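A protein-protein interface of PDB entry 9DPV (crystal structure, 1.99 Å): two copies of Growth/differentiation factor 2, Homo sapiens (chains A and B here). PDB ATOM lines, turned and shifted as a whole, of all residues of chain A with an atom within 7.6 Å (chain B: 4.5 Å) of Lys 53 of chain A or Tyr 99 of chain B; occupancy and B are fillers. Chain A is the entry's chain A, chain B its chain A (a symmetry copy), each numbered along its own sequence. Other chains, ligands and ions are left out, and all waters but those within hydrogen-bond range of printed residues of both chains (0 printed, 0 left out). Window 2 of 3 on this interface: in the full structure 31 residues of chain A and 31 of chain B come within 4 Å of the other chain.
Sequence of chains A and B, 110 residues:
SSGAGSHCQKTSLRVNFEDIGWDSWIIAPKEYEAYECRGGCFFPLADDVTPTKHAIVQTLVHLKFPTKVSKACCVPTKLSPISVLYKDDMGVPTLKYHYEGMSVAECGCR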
ATOM      1  N   THR A  50     -31.738  -0.878  19.487  1.00  0.00           N
ATOM      2  CA  THR A  50     -30.621   0.024  19.214  1.00  0.00           C
ATOM      3  C   THR A  50     -30.712   1.313  20.041  1.00  0.00           C
ATOM      4  O   THR A  50     -30.696   2.413  19.480  1.00  0.00           O
ATOM      5  CB  THR A  50     -30.529   0.342  17.726  1.00  0.00           C
ATOM      6  OG1 THR A  50     -31.659   1.133  17.352  1.00  0.00           O
ATOM      7  CG2 THR A  50     -30.512  -0.948  16.894  1.00  0.00           C
ATOM      8  N   PRO A  51     -30.807   1.208  21.367  1.00  0.00           N
ATOM      9  CA  PRO A  51     -31.104   2.402  22.166  1.00  0.00           C
ATOM     10  C   PRO A  51     -29.887   3.310  22.279  1.00  0.00           C
ATOM     11  O   PRO A  51     -28.788   2.866  22.621  1.00  0.00           O
ATOM     12  CB  PRO A  51     -31.503   1.826  23.528  1.00  0.00           C
ATOM     13  CG  PRO A  51     -30.731   0.563  23.627  1.00  0.00           C
ATOM     14  CD  PRO A  51     -30.600   0.020  22.218  1.00  0.00           C
ATOM     15  N   THR A  52     -30.090   4.588  21.970  1.00  0.00           N
ATOM     16  CA  THR A  52     -29.096   5.600  22.282  1.00  0.00           C
ATOM     17  C   THR A  52     -28.897   5.677  23.797  1.00  0.00           C
ATOM     18  O   THR A  52     -29.736   5.232  24.584  1.00  0.00           O
ATOM     19  CB  THR A  52     -29.538   6.967  21.756  1.00  0.00           C
ATOM     20  OG1 THR A  52     -30.777   7.312  22.380  1.00  0.00           O
ATOM     21  CG2 THR A  52     -29.721   6.979  20.214  1.00  0.00           C
ATOM     22  N   LYS A  53     -27.762   6.252  24.204  1.00  0.00           N
ATOM     23  CA  LYS A  53     -27.524   6.482  25.614  1.00  0.00           C
ATOM     24  C   LYS A  53     -28.558   7.446  26.196  1.00  0.00           C
ATOM     25  O   LYS A  53     -28.992   7.275  27.331  1.00  0.00           O
ATOM     26  CB  LYS A  53     -26.094   6.997  25.855  1.00  0.00           C
ATOM     27  CG  LYS A  53     -24.984   6.004  25.460  1.00  0.00           C
ATOM     28  CD  LYS A  53     -23.605   6.401  25.984  1.00  0.00           C
ATOM     29  CE  LYS A  53     -22.435   5.698  25.289  1.00  0.00           C
ATOM     30  NZ  LYS A  53     -22.178   6.187  23.903  1.00  0.00           N
ATOM     31  N   HIS A  54     -28.967   8.462  25.424  1.00  0.00           N
ATOM     32  CA  HIS A  54     -29.962   9.405  25.919  1.00  0.00           C
ATOM     33  C   HIS A  54     -31.287   8.709  26.232  1.00  0.00           C
ATOM     34  O   HIS A  54     -31.866   8.931  27.289  1.00  0.00           O
ATOM     35  CB  HIS A  54     -30.184  10.590  24.960  1.00  0.00           C
ATOM     36  CG  HIS A  54     -30.948  11.696  25.623  1.00  0.00           C
ATOM     37  ND1 HIS A  54     -32.327  11.639  25.771  1.00  0.00           N
ATOM     38  CD2 HIS A  54     -30.496  12.831  26.198  1.00  0.00           C
ATOM     39  CE1 HIS A  54     -32.664  12.730  26.443  1.00  0.00           C
ATOM     40  NE2 HIS A  54     -31.587  13.478  26.715  1.00  0.00           N
ATOM     41  N   ALA A  55     -31.744   7.831  25.335  1.00  0.00           N
ATOM     42  CA  ALA A  55     -32.955   7.050  25.578  1.00  0.00           C
ATOM     43  C   ALA A  55     -32.885   6.198  26.849  1.00  0.00           C
ATOM     44  O   ALA A  55     -33.861   6.068  27.588  1.00  0.00           O
ATOM     45  CB  ALA A  55     -33.230   6.166  24.380  1.00  0.00           C
ATOM     46  N   ILE A  56     -31.707   5.626  27.114  1.00  0.00           N
ATOM     47  CA  ILE A  56     -31.492   4.840  28.317  1.00  0.00           C
ATOM     48  C   ILE A  56     -31.569   5.724  29.559  1.00  0.00           C
ATOM     49  O   ILE A  56     -32.290   5.415  30.505  1.00  0.00           O
ATOM     50  CB  ILE A  56     -30.142   4.077  28.189  1.00  0.00           C
ATOM     51  CG1 ILE A  56     -30.237   3.031  27.055  1.00  0.00           C
ATOM     52  CG2 ILE A  56     -29.737   3.447  29.479  1.00  0.00           C
ATOM     53  CD1 ILE A  56     -28.922   2.408  26.640  1.00  0.00           C
ATOM     54  N   VAL A  57     -30.821   6.832  29.544  1.00  0.00           N
ATOM     55  CA  VAL A  57     -30.818   7.775  30.652  1.00  0.00           C
ATOM     56  C   VAL A  57     -32.207   8.342  30.938  1.00  0.00           C
ATOM     57  O   VAL A  57     -32.643   8.402  32.082  1.00  0.00           O
ATOM     58  CB  VAL A  57     -29.811   8.895  30.364  1.00  0.00           C
ATOM     59  CG1 VAL A  57     -30.053  10.112  31.241  1.00  0.00           C
ATOM     60  CG2 VAL A  57     -28.394   8.377  30.518  1.00  0.00           C
ATOM     61  N   GLN A  58     -32.908   8.756  29.882  1.00  0.00           N
ATOM     62  CA  GLN A  58     -34.233   9.317  30.064  1.00  0.00           C
ATOM     63  C   GLN A  58     -35.206   8.295  30.645  1.00  0.00           C
ATOM     64  O   GLN A  58     -35.993   8.616  31.529  1.00  0.00           O
ATOM     65  CB  GLN A  58     -34.756   9.895  28.731  1.00  0.00           C
ATOM     66  CG  GLN A  58     -36.066  10.606  28.953  1.00  0.00           C
ATOM     67  CD  GLN A  58     -36.494  11.455  27.809  1.00  0.00           C
ATOM     68  OE1 GLN A  58     -35.681  11.963  27.051  1.00  0.00           O
ATOM     69  NE2 GLN A  58     -37.801  11.620  27.693  1.00  0.00           N
ATOM     70  N   THR A  59     -35.127   7.048  30.171  1.00  0.00           N
ATOM     71  CA  THR A  59     -35.961   5.981  30.703  1.00  0.00           C
ATOM     72  C   THR A  59     -35.732   5.754  32.197  1.00  0.00           C
ATOM     73  O   THR A  59     -36.687   5.552  32.947  1.00  0.00           O
ATOM     74  CB  THR A  59     -35.741   4.709  29.891  1.00  0.00           C
ATOM     75  OG1 THR A  59     -35.984   5.007  28.506  1.00  0.00           O
ATOM     76  CG2 THR A  59     -36.642   3.551  30.359  1.00  0.00           C
ATOM     77  N   LEU A  60     -34.464   5.801  32.624  1.00  0.00           N
ATOM     78  CA  LEU A  60     -34.129   5.685  34.035  1.00  0.00           C
ATOM     79  C   LEU A  60     -34.626   6.878  34.847  1.00  0.00           C
ATOM     80  O   LEU A  60     -35.124   6.713  35.955  1.00  0.00           O
ATOM     81  CB  LEU A  60     -32.606   5.543  34.201  1.00  0.00           C
ATOM     82  CG  LEU A  60     -32.009   4.223  33.685  1.00  0.00           C
ATOM     83  CD1 LEU A  60     -30.486   4.267  33.701  1.00  0.00           C
ATOM     84  CD2 LEU A  60     -32.494   3.055  34.503  1.00  0.00           C
ATOM     85  N   CYS A 109     -35.873   2.780  20.179  1.00  0.00           N
ATOM     86  CA  CYS A 109     -36.173   3.683  21.276  1.00  0.00           C
ATOM     87  C   CYS A 109     -35.233   4.883  21.216  1.00  0.00           C
ATOM     88  O   CYS A 109     -34.023   4.706  21.097  1.00  0.00           O
ATOM     89  CB  CYS A 109     -36.057   2.925  22.597  1.00  0.00           C
ATOM     90  SG  CYS A 109     -37.308   1.628  22.780  1.00  0.00           S
ATOM     91  N   ARG A 110     -35.816   6.089  21.262  1.00  0.00           N
ATOM     92  CA  ARG A 110     -35.089   7.335  21.095  1.00  0.00           C
ATOM     93  C   ARG A 110     -35.556   8.369  22.124  1.00  0.00           C
ATOM     94  O   ARG A 110     -34.772   9.231  22.542  1.00  0.00           O
ATOM     95  CB  ARG A 110     -35.269   7.864  19.666  1.00  0.00           C
ATOM     96  CG  ARG A 110     -34.628   6.988  18.610  1.00  0.00           C
ATOM     97  CD  ARG A 110     -33.124   6.945  18.756  1.00  0.00           C
ATOM     98  NE  ARG A 110     -32.484   6.145  17.720  1.00  0.00           N
ATOM     99  CZ  ARG A 110     -32.267   4.838  17.790  1.00  0.00           C
ATOM    100  NH1 ARG A 110     -32.763   4.099  18.771  1.00  0.00           N
ATOM    101  NH2 ARG A 110     -31.540   4.255  16.843  1.00  0.00           N
ATOM    102  OXT ARG A 110     -36.707   8.332  22.552  1.00  0.00           O
ATOM    103  N   TRP B  25     -20.131   3.642  38.584  1.00  0.00           N
ATOM    104  CA  TRP B  25     -19.026   3.651  37.635  1.00  0.00           C
ATOM    105  C   TRP B  25     -18.597   5.041  37.164  1.00  0.00           C
ATOM    106  O   TRP B  25     -17.430   5.230  36.837  1.00  0.00           O
ATOM    107  CB  TRP B  25     -19.327   2.730  36.432  1.00  0.00           C
ATOM    108  CG  TRP B  25     -20.276   3.270  35.410  1.00  0.00           C
ATOM    109  CD1 TRP B  25     -21.632   3.377  35.509  1.00  0.00           C
ATOM    110  CD2 TRP B  25     -19.927   3.771  34.117  1.00  0.00           C
ATOM    111  NE1 TRP B  25     -22.150   3.918  34.352  1.00  0.00           N
ATOM    112  CE2 TRP B  25     -21.123   4.168  33.481  1.00  0.00           C
ATOM    113  CE3 TRP B  25     -18.716   3.923  33.432  1.00  0.00           C
ATOM    114  CZ2 TRP B  25     -21.136   4.710  32.197  1.00  0.00           C
ATOM    115  CZ3 TRP B  25     -18.733   4.461  32.162  1.00  0.00           C
ATOM    116  CH2 TRP B  25     -19.930   4.846  31.557  1.00  0.00           C
ATOM    117  N   PRO B  81     -21.935  14.517  22.657  1.00  0.00           N
ATOM    118  CA  PRO B  81     -21.220  13.851  23.737  1.00  0.00           C
ATOM    119  C   PRO B  81     -21.024  14.727  24.969  1.00  0.00           C
ATOM    120  O   PRO B  81     -21.186  15.944  24.914  1.00  0.00           O
ATOM    121  CB  PRO B  81     -19.877  13.526  23.093  1.00  0.00           C
ATOM    122  CG  PRO B  81     -19.657  14.692  22.142  1.00  0.00           C
ATOM    123  CD  PRO B  81     -21.038  15.043  21.617  1.00  0.00           C
ATOM    124  N   ILE B  82     -20.668  14.073  26.078  1.00  0.00           N
ATOM    125  CA  ILE B  82     -20.128  14.733  27.250  1.00  0.00           C
ATOM    126  C   ILE B  82     -18.874  13.957  27.638  1.00  0.00           C
ATOM    127  O   ILE B  82     -18.638  12.857  27.142  1.00  0.00           O
ATOM    128  CB  ILE B  82     -21.127  14.800  28.421  1.00  0.00           C
ATOM    129  CG1 ILE B  82     -21.431  13.387  29.001  1.00  0.00           C
ATOM    130  CG2 ILE B  82     -22.411  15.518  28.021  1.00  0.00           C
ATOM    131  CD1 ILE B  82     -22.006  13.417  30.371  1.00  0.00           C
ATOM    132  N   VAL B  84     -16.932  12.043  30.719  1.00  0.00           N
ATOM    133  CA  VAL B  84     -17.110  11.439  32.026  1.00  0.00           C
ATOM    134  C   VAL B  84     -15.778  10.892  32.537  1.00  0.00           C
ATOM    135  O   VAL B  84     -14.954  10.409  31.759  1.00  0.00           O
ATOM    136  CB  VAL B  84     -18.204  10.359  31.977  1.00  0.00           C
ATOM    137  CG1 VAL B  84     -19.561  10.978  31.633  1.00  0.00           C
ATOM    138  CG2 VAL B  84     -17.850   9.238  31.004  1.00  0.00           C
ATOM    139  N   LYS B  96     -13.177   9.582  29.775  1.00  0.00           N
ATOM    140  CA  LYS B  96     -13.782   9.245  28.499  1.00  0.00           C
ATOM    141  C   LYS B  96     -14.186  10.564  27.840  1.00  0.00           C
ATOM    142  O   LYS B  96     -15.205  11.150  28.180  1.00  0.00           O
ATOM    143  CB  LYS B  96     -14.956   8.287  28.714  1.00  0.00           C
ATOM    144  CG  LYS B  96     -15.767   7.984  27.471  1.00  0.00           C
ATOM    145  CD  LYS B  96     -14.932   7.490  26.308  1.00  0.00           C
ATOM    146  CE  LYS B  96     -15.793   7.226  25.105  1.00  0.00           C
ATOM    147  NZ  LYS B  96     -14.980   7.051  23.883  1.00  0.00           N
ATOM    148  N   TYR B  97     -13.359  11.042  26.909  1.00  0.00           N
ATOM    149  CA  TYR B  97     -13.425  12.434  26.500  1.00  0.00           C
ATOM    150  C   TYR B  97     -14.714  12.739  25.740  1.00  0.00           C
ATOM    151  O   TYR B  97     -15.412  13.680  26.092  1.00  0.00           O
ATOM    152  CB  TYR B  97     -12.192  12.812  25.693  1.00  0.00           C
ATOM    153  CG  TYR B  97     -12.124  14.283  25.363  1.00  0.00           C
ATOM    154  CD1 TYR B  97     -12.143  15.245  26.366  1.00  0.00           C
ATOM    155  CD2 TYR B  97     -12.034  14.715  24.051  1.00  0.00           C
ATOM    156  CE1 TYR B  97     -12.074  16.601  26.068  1.00  0.00           C
ATOM    157  CE2 TYR B  97     -11.965  16.065  23.741  1.00  0.00           C
ATOM    158  CZ  TYR B  97     -11.981  17.008  24.753  1.00  0.00           C
ATOM    159  OH  TYR B  97     -11.933  18.343  24.446  1.00  0.00           O
ATOM    160  N   HIS B  98     -15.037  11.917  24.737  1.00  0.00           N
ATOM    161  CA  HIS B  98     -16.321  11.997  24.053  1.00  0.00           C
ATOM    162  C   HIS B  98     -17.189  10.763  24.302  1.00  0.00           C
ATOM    163  O   HIS B  98     -17.183   9.818  23.514  1.00  0.00           O
ATOM    164  CB  HIS B  98     -16.132  12.194  22.539  1.00  0.00           C
ATOM    165  CG  HIS B  98     -15.413  13.453  22.153  1.00  0.00           C
ATOM    166  ND1 HIS B  98     -15.816  14.689  22.615  1.00  0.00           N
ATOM    167  CD2 HIS B  98     -14.330  13.617  21.361  1.00  0.00           C
ATOM    168  CE1 HIS B  98     -14.971  15.567  22.089  1.00  0.00           C
ATOM    169  NE2 HIS B  98     -14.059  14.958  21.327  1.00  0.00           N
ATOM    170  N   TYR B  99     -17.966  10.801  25.388  1.00  0.00           N
ATOM    171  CA  TYR B  99     -18.946   9.764  25.674  1.00  0.00           C
ATOM    172  C   TYR B  99     -20.214  10.089  24.891  1.00  0.00           C
ATOM    173  O   TYR B  99     -21.008  10.926  25.314  1.00  0.00           O
ATOM    174  CB  TYR B  99     -19.206   9.677  27.185  1.00  0.00           C
ATOM    175  CG  TYR B  99     -19.848   8.383  27.639  1.00  0.00           C
ATOM    176  CD1 TYR B  99     -19.279   7.155  27.329  1.00  0.00           C
ATOM    177  CD2 TYR B  99     -21.006   8.389  28.404  1.00  0.00           C
ATOM    178  CE1 TYR B  99     -19.854   5.964  27.757  1.00  0.00           C
ATOM    179  CE2 TYR B  99     -21.595   7.202  28.833  1.00  0.00           C
ATOM    180  CZ  TYR B  99     -21.016   5.992  28.506  1.00  0.00           C
ATOM    181  OH  TYR B  99     -21.579   4.811  28.925  1.00  0.00           O
ATOM    182  N   GLU B 100     -20.385   9.416  23.746  1.00  0.00           N
ATOM    183  CA  GLU B 100     -21.339   9.834  22.734  1.00  0.00           C
ATOM    184  C   GLU B 100     -22.799   9.570  23.101  1.00  0.00           C
ATOM    185  O   GLU B 100     -23.130   8.602  23.784  1.00  0.00           O
ATOM    186  CB  GLU B 100     -21.025   9.131  21.402  1.00  0.00           C
ATOM    187  CG  GLU B 100     -19.638   9.432  20.849  1.00  0.00           C
ATOM    188  CD  GLU B 100     -19.431  10.829  20.289  1.00  0.00           C
ATOM    189  OE1 GLU B 100     -20.429  11.565  20.110  1.00  0.00           O
ATOM    190  OE2 GLU B 100     -18.260  11.185  20.025  1.00  0.00           O
ATOM    191  N   GLY B 101     -23.667  10.470  22.642  1.00  0.00           N
ATOM    192  CA  GLY B 101     -25.099  10.238  22.637  1.00  0.00           C
ATOM    193  C   GLY B 101     -25.784  10.616  23.943  1.00  0.00           C
ATOM    194  O   GLY B 101     -26.876  10.132  24.219  1.00  0.00           O
ATOM    195  N   MET B 102     -25.145  11.491  24.727  1.00  0.00           N
ATOM    196  CA  MET B 102     -25.595  11.761  26.082  1.00  0.00           C
ATOM    197  C   MET B 102     -26.516  12.972  26.238  1.00  0.00           C
ATOM    198  O   MET B 102     -27.281  13.038  27.197  1.00  0.00           O
ATOM    199  CB  MET B 102     -24.367  11.917  26.976  1.00  0.00           C
ATOM    200  CG  MET B 102     -23.681  10.596  27.239  1.00  0.00           C
ATOM    201  SD  MET B 102     -24.677   9.466  28.202  1.00  0.00           S
ATOM    202  CE  MET B 102     -24.500  10.158  29.814  1.00  0.00           C
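The backbone carbonyl oxygen (O) of Ile 82 of chain B sits at hydrogen-bond distance from the backbone NH (N) of Tyr 99 of chain B, 2.8 Å away.
O of Glu 100 of chain B sits at hydrogen-bond distance from NZ of Lys 53 of chain A (2.6 Å). N of His 54 of chain A sits at hydrogen-bond distance from O of Gly 101 of chain B (2.9 Å).
Printed residues of chain A that touch a printed residue of chain B: Lys 53 and His 54. Of the 11 printed residues of chain B, 4 touch a printed residue of chain A. Hydrophobic or aromatic side chains of chain B that line the printed part of chain A: Tyr 99 and Met 102. Among the printed residues, 6 pairs touch across the chains. Among the printed residues, no Asp or Glu carboxylate lies within 4 Å of a Lys or Arg side-chain nitrogen of the other chain.
Among the printed residues, merely in contact across the chains: Lys 53 of chain A with Tyr 99 of chain B (3.5 Å), Lys 53 of chain A with Gly 101 of chain B (3.6 Å), Lys 53 of chain A with Met 102 of chain B (3.7 Å) and His 54 of chain A with Met 102 of chain B (3.4 Å).
Of the printed residues of chain B, His 54 of chain A touches Gly 101 and Met 102. Leu 60 of chain A touches none of the printed residues of chain B. Pro 81 of chain B touches none of the printed residues of chain A. Tyr 99 of chain B touches one residue of chain A. Of the printed residues of chain A, Met 102 of chain B touches Lys 53 (3.7 Å) and His 54 (3.4 Å). The nearest printed residue of chain B that does not touch Lys 53 of chain A is His 98 of chain B (6.2 Å). The nearest printed residue of chain A that does not touch Gly 101 of chain B is Thr 52 of chain A (4.8 Å).
No position is printed for both chains.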
